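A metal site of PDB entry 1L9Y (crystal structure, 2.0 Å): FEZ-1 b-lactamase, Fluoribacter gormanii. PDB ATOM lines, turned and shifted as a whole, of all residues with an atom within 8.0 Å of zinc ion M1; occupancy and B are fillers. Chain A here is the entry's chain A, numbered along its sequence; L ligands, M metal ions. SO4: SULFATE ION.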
ATOM      1  N   SER A  70      30.199  10.360 -12.111  1.00  0.00           N
ATOM      2  CA  SER A  70      29.025  10.589 -11.275  1.00  0.00           C
ATOM      3  C   SER A  70      27.812  10.802 -12.177  1.00  0.00           C
ATOM      4  O   SER A  70      26.748  10.238 -11.948  1.00  0.00           O
ATOM      5  CB  SER A  70      29.232  11.811 -10.367  1.00  0.00           C
ATOM      6  OG  SER A  70      30.256  11.587  -9.420  1.00  0.00           O
ATOM      7  N   HIS A  71      27.972  11.639 -13.193  1.00  0.00           N
ATOM      8  CA  HIS A  71      26.893  11.898 -14.155  1.00  0.00           C
ATOM      9  C   HIS A  71      27.438  12.576 -15.406  1.00  0.00           C
ATOM     10  O   HIS A  71      28.528  13.175 -15.378  1.00  0.00           O
ATOM     11  CB  HIS A  71      25.752  12.722 -13.539  1.00  0.00           C
ATOM     12  CG  HIS A  71      26.113  14.134 -13.199  1.00  0.00           C
ATOM     13  ND1 HIS A  71      26.448  14.532 -11.931  1.00  0.00           N
ATOM     14  CD2 HIS A  71      26.151  15.246 -13.972  1.00  0.00           C
ATOM     15  CE1 HIS A  71      26.680  15.826 -11.925  1.00  0.00           C
ATOM     16  NE2 HIS A  71      26.513  16.295 -13.154  1.00  0.00           N
ATOM     17  N   ALA A  72      26.689  12.486 -16.492  1.00  0.00           N
ATOM     18  CA  ALA A  72      27.129  13.046 -17.772  1.00  0.00           C
ATOM     19  C   ALA A  72      26.938  14.541 -18.001  1.00  0.00           C
ATOM     20  O   ALA A  72      25.959  14.959 -18.625  1.00  0.00           O
ATOM     21  CB  ALA A  72      26.480  12.262 -18.922  1.00  0.00           C
ATOM     22  N   HIS A  73      27.879  15.310 -17.481  1.00  0.00           N
ATOM     23  CA  HIS A  73      27.924  16.764 -17.638  1.00  0.00           C
ATOM     24  C   HIS A  73      29.422  17.071 -17.808  1.00  0.00           C
ATOM     25  O   HIS A  73      30.264  16.440 -17.170  1.00  0.00           O
ATOM     26  CB  HIS A  73      27.343  17.483 -16.407  1.00  0.00           C
ATOM     27  CG  HIS A  73      25.867  17.720 -16.498  1.00  0.00           C
ATOM     28  ND1 HIS A  73      25.113  18.163 -15.438  1.00  0.00           N
ATOM     29  CD2 HIS A  73      25.006  17.593 -17.542  1.00  0.00           C
ATOM     30  CE1 HIS A  73      23.855  18.304 -15.821  1.00  0.00           C
ATOM     31  NE2 HIS A  73      23.761  17.958 -17.096  1.00  0.00           N
ATOM     32  N   PHE A  74      29.749  18.018 -18.685  1.00  0.00           N
ATOM     33  CA  PHE A  74      31.149  18.348 -18.966  1.00  0.00           C
ATOM     34  C   PHE A  74      32.085  18.472 -17.759  1.00  0.00           C
ATOM     35  O   PHE A  74      33.229  18.030 -17.830  1.00  0.00           O
ATOM     36  CB  PHE A  74      31.219  19.635 -19.803  1.00  0.00           C
ATOM     37  CG  PHE A  74      30.936  20.876 -19.008  1.00  0.00           C
ATOM     38  CD1 PHE A  74      31.976  21.553 -18.365  1.00  0.00           C
ATOM     39  CD2 PHE A  74      29.637  21.336 -18.851  1.00  0.00           C
ATOM     40  CE1 PHE A  74      31.712  22.662 -17.570  1.00  0.00           C
ATOM     41  CE2 PHE A  74      29.370  22.446 -18.042  1.00  0.00           C
ATOM     42  CZ  PHE A  74      30.411  23.110 -17.405  1.00  0.00           C
ATOM     43  N   ASP A  75      31.626  19.070 -16.666  1.00  0.00           N
ATOM     44  CA  ASP A  75      32.512  19.234 -15.517  1.00  0.00           C
ATOM     45  C   ASP A  75      32.910  17.934 -14.812  1.00  0.00           C
ATOM     46  O   ASP A  75      33.787  17.933 -13.959  1.00  0.00           O
ATOM     47  CB  ASP A  75      31.925  20.214 -14.502  1.00  0.00           C
ATOM     48  CG  ASP A  75      30.587  19.775 -13.966  1.00  0.00           C
ATOM     49  OD1 ASP A  75      30.259  20.175 -12.835  1.00  0.00           O
ATOM     50  OD2 ASP A  75      29.849  19.045 -14.668  1.00  0.00           O
ATOM     51  N   HIS A  76      32.265  16.831 -15.182  1.00  0.00           N
ATOM     52  CA  HIS A  76      32.588  15.551 -14.561  1.00  0.00           C
ATOM     53  C   HIS A  76      33.099  14.526 -15.561  1.00  0.00           C
ATOM     54  O   HIS A  76      33.817  13.594 -15.182  1.00  0.00           O
ATOM     55  CB  HIS A  76      31.366  14.986 -13.829  1.00  0.00           C
ATOM     56  CG  HIS A  76      30.854  15.891 -12.763  1.00  0.00           C
ATOM     57  ND1 HIS A  76      31.597  16.233 -11.660  1.00  0.00           N
ATOM     58  CD2 HIS A  76      29.706  16.609 -12.678  1.00  0.00           C
ATOM     59  CE1 HIS A  76      30.938  17.128 -10.939  1.00  0.00           C
ATOM     60  NE2 HIS A  76      29.788  17.373 -11.539  1.00  0.00           N
ATOM     61  N   ASP A 108      22.018  16.236 -24.757  1.00  0.00           N
ATOM     62  CA  ASP A 108      21.609  16.610 -23.402  1.00  0.00           C
ATOM     63  C   ASP A 108      20.207  17.195 -23.423  1.00  0.00           C
ATOM     64  O   ASP A 108      19.948  18.159 -24.143  1.00  0.00           O
ATOM     65  CB  ASP A 108      22.606  17.611 -22.800  1.00  0.00           C
ATOM     66  CG  ASP A 108      22.386  17.843 -21.319  1.00  0.00           C
ATOM     67  OD1 ASP A 108      21.385  18.484 -20.955  1.00  0.00           O
ATOM     68  OD2 ASP A 108      23.216  17.370 -20.520  1.00  0.00           O
ATOM     69  N   TYR A 111      20.947  20.967 -22.164  1.00  0.00           N
ATOM     70  CA  TYR A 111      21.980  21.750 -22.839  1.00  0.00           C
ATOM     71  C   TYR A 111      22.294  21.392 -24.289  1.00  0.00           C
ATOM     72  O   TYR A 111      23.304  21.853 -24.836  1.00  0.00           O
ATOM     73  CB  TYR A 111      23.283  21.671 -22.021  1.00  0.00           C
ATOM     74  CG  TYR A 111      23.120  22.074 -20.576  1.00  0.00           C
ATOM     75  CD1 TYR A 111      23.262  21.140 -19.543  1.00  0.00           C
ATOM     76  CD2 TYR A 111      22.801  23.386 -20.231  1.00  0.00           C
ATOM     77  CE1 TYR A 111      23.098  21.508 -18.204  1.00  0.00           C
ATOM     78  CE2 TYR A 111      22.640  23.766 -18.900  1.00  0.00           C
ATOM     79  CZ  TYR A 111      22.788  22.830 -17.894  1.00  0.00           C
ATOM     80  OH  TYR A 111      22.627  23.196 -16.570  1.00  0.00           O
ATOM     81  N   HIS A 149      19.018  15.003 -12.157  1.00  0.00           N
ATOM     82  CA  HIS A 149      20.061  15.952 -12.536  1.00  0.00           C
ATOM     83  C   HIS A 149      20.487  15.629 -13.979  1.00  0.00           C
ATOM     84  O   HIS A 149      20.736  16.520 -14.782  1.00  0.00           O
ATOM     85  CB  HIS A 149      21.251  15.829 -11.595  1.00  0.00           C
ATOM     86  CG  HIS A 149      22.238  16.921 -11.759  1.00  0.00           C
ATOM     87  ND1 HIS A 149      21.987  18.218 -11.353  1.00  0.00           N
ATOM     88  CD2 HIS A 149      23.463  16.934 -12.339  1.00  0.00           C
ATOM     89  CE1 HIS A 149      23.005  18.983 -11.681  1.00  0.00           C
ATOM     90  NE2 HIS A 149      23.914  18.233 -12.276  1.00  0.00           N
ATOM     91  N   THR A 150      20.603  14.335 -14.262  1.00  0.00           N
ATOM     92  CA  THR A 150      20.876  13.830 -15.609  1.00  0.00           C
ATOM     93  C   THR A 150      20.058  12.548 -15.648  1.00  0.00           C
ATOM     94  O   THR A 150      19.690  12.019 -14.601  1.00  0.00           O
ATOM     95  CB  THR A 150      22.374  13.491 -15.890  1.00  0.00           C
ATOM     96  OG1 THR A 150      22.788  12.358 -15.122  1.00  0.00           O
ATOM     97  CG2 THR A 150      23.279  14.690 -15.601  1.00  0.00           C
ATOM     98  N   CYS A 153      22.270   9.881 -13.854  1.00  0.00           N
ATOM     99  CA  CYS A 153      23.110  10.264 -12.725  1.00  0.00           C
ATOM    100  C   CYS A 153      23.320   9.074 -11.803  1.00  0.00           C
ATOM    101  O   CYS A 153      22.367   8.436 -11.353  1.00  0.00           O
ATOM    102  CB  CYS A 153      22.494  11.415 -11.941  1.00  0.00           C
ATOM    103  SG  CYS A 153      23.531  11.919 -10.544  1.00  0.00           S
ATOM    104  N   GLY A 173      25.944  11.422  -6.657  1.00  0.00           N
ATOM    105  CA  GLY A 173      26.087  11.935  -8.016  1.00  0.00           C
ATOM    106  C   GLY A 173      25.667  13.371  -8.190  1.00  0.00           C
ATOM    107  O   GLY A 173      26.333  14.135  -8.896  1.00  0.00           O
ATOM    108  N   SER A 174      24.547  13.726  -7.540  1.00  0.00           N
ATOM    109  CA  SER A 174      23.937  15.056  -7.553  1.00  0.00           C
ATOM    110  C   SER A 174      22.437  14.994  -7.795  1.00  0.00           C
ATOM    111  O   SER A 174      21.988  14.325  -8.712  1.00  0.00           O
ATOM    112  CB  SER A 174      24.541  15.964  -8.633  1.00  0.00           C
ATOM    113  OG  SER A 174      23.836  17.202  -8.683  1.00  0.00           O
ATOM    114  N   GLY A 176      20.820  18.066  -7.543  1.00  0.00           N
ATOM    115  CA  GLY A 176      20.587  19.500  -7.602  1.00  0.00           C
ATOM    116  C   GLY A 176      19.829  19.846  -8.861  1.00  0.00           C
ATOM    117  O   GLY A 176      19.952  19.172  -9.895  1.00  0.00           O
ATOM    118  N   ASN A 178      19.522  22.298 -11.805  1.00  0.00           N
ATOM    119  CA  ASN A 178      20.265  23.354 -12.487  1.00  0.00           C
ATOM    120  C   ASN A 178      19.342  24.476 -12.948  1.00  0.00           C
ATOM    121  O   ASN A 178      18.222  24.245 -13.403  1.00  0.00           O
ATOM    122  CB  ASN A 178      21.014  22.816 -13.694  1.00  0.00           C
ATOM    123  CG  ASN A 178      22.342  22.174 -13.337  1.00  0.00           C
ATOM    124  OD1 ASN A 178      22.819  22.274 -12.196  1.00  0.00           O
ATOM    125  ND2 ASN A 178      22.960  21.511 -14.303  1.00  0.00           N
ATOM    126  N   SER A 214      30.164  14.563  -6.022  1.00  0.00           N
ATOM    127  CA  SER A 214      30.820  14.954  -7.262  1.00  0.00           C
ATOM    128  C   SER A 214      31.493  16.311  -7.124  1.00  0.00           C
ATOM    129  O   SER A 214      32.395  16.645  -7.896  1.00  0.00           O
ATOM    130  CB  SER A 214      29.817  14.955  -8.413  1.00  0.00           C
ATOM    131  OG  SER A 214      28.628  15.648  -8.052  1.00  0.00           O
ATOM    132  N   HIS A 215      31.049  17.097  -6.142  1.00  0.00           N
ATOM    133  CA  HIS A 215      31.618  18.426  -5.895  1.00  0.00           C
ATOM    134  C   HIS A 215      32.107  18.529  -4.446  1.00  0.00           C
ATOM    135  O   HIS A 215      31.404  18.112  -3.520  1.00  0.00           O
ATOM    136  CB  HIS A 215      30.584  19.515  -6.139  1.00  0.00           C
ATOM    137  CG  HIS A 215      30.360  19.816  -7.586  1.00  0.00           C
ATOM    138  ND1 HIS A 215      31.122  20.722  -8.296  1.00  0.00           N
ATOM    139  CD2 HIS A 215      29.453  19.326  -8.468  1.00  0.00           C
ATOM    140  CE1 HIS A 215      30.698  20.777  -9.538  1.00  0.00           C
ATOM    141  NE2 HIS A 215      29.683  19.938  -9.676  1.00  0.00           N
ATOM    142  N   MET A 218      29.886  19.947  -1.691  1.00  0.00           N
ATOM    143  CA  MET A 218      28.765  19.135  -1.230  1.00  0.00           C
ATOM    144  C   MET A 218      29.018  18.561   0.150  1.00  0.00           C
ATOM    145  O   MET A 218      28.111  18.539   0.993  1.00  0.00           O
ATOM    146  CB  MET A 218      28.502  17.974  -2.192  1.00  0.00           C
ATOM    147  CG  MET A 218      28.067  18.360  -3.585  1.00  0.00           C
ATOM    148  SD  MET A 218      27.852  16.901  -4.622  1.00  0.00           S
ATOM    149  CE  MET A 218      26.889  17.562  -5.995  1.00  0.00           C
HETATM  150  S   SO4 L   1      26.592  21.718 -12.766  1.00  0.00           S
HETATM  151  O1  SO4 L   1      27.392  22.340 -13.845  1.00  0.00           O
HETATM  152  O2  SO4 L   1      25.794  22.758 -12.087  1.00  0.00           O
HETATM  153  O3  SO4 L   1      27.495  21.112 -11.795  1.00  0.00           O
HETATM  154  O4  SO4 L   1      25.684  20.718 -13.341  1.00  0.00           O
HETATM  155 ZN    ZN M   1      25.743  18.403 -13.371  1.00  0.00          ZN
HETATM  156 ZN    ZN M   2      28.727  19.284 -11.502  1.00  0.00          ZN
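Zinc ion M1 is bound by NE2 of His 149 (2.1 Å).
ND1 of His 73 binds zinc ion M1, 2.2 Å away.
Zinc ion M1 is bound by NE2 of His 71 (2.3 Å).
O4 of the ligand is bound to zinc ion M1 (2.3 Å).
Of the 19 residues printed, 3 come within 4 Å of zinc ion M1.
A ring nitrogen (ND1) of His 71 sits at hydrogen-bond distance from the backbone carbonyl oxygen (O) of Gly 173 (3.1 Å).
A ring nitrogen (ND1) of His 149 lies within hydrogen-bond range of the backbone carbonyl oxygen (O) of Gly 176, 2.7 Å away.
A ring nitrogen (ND1) of His 149 sits at hydrogen-bond distance from the side-chain hydroxyl (OG) of Ser 174 (3.4 Å).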
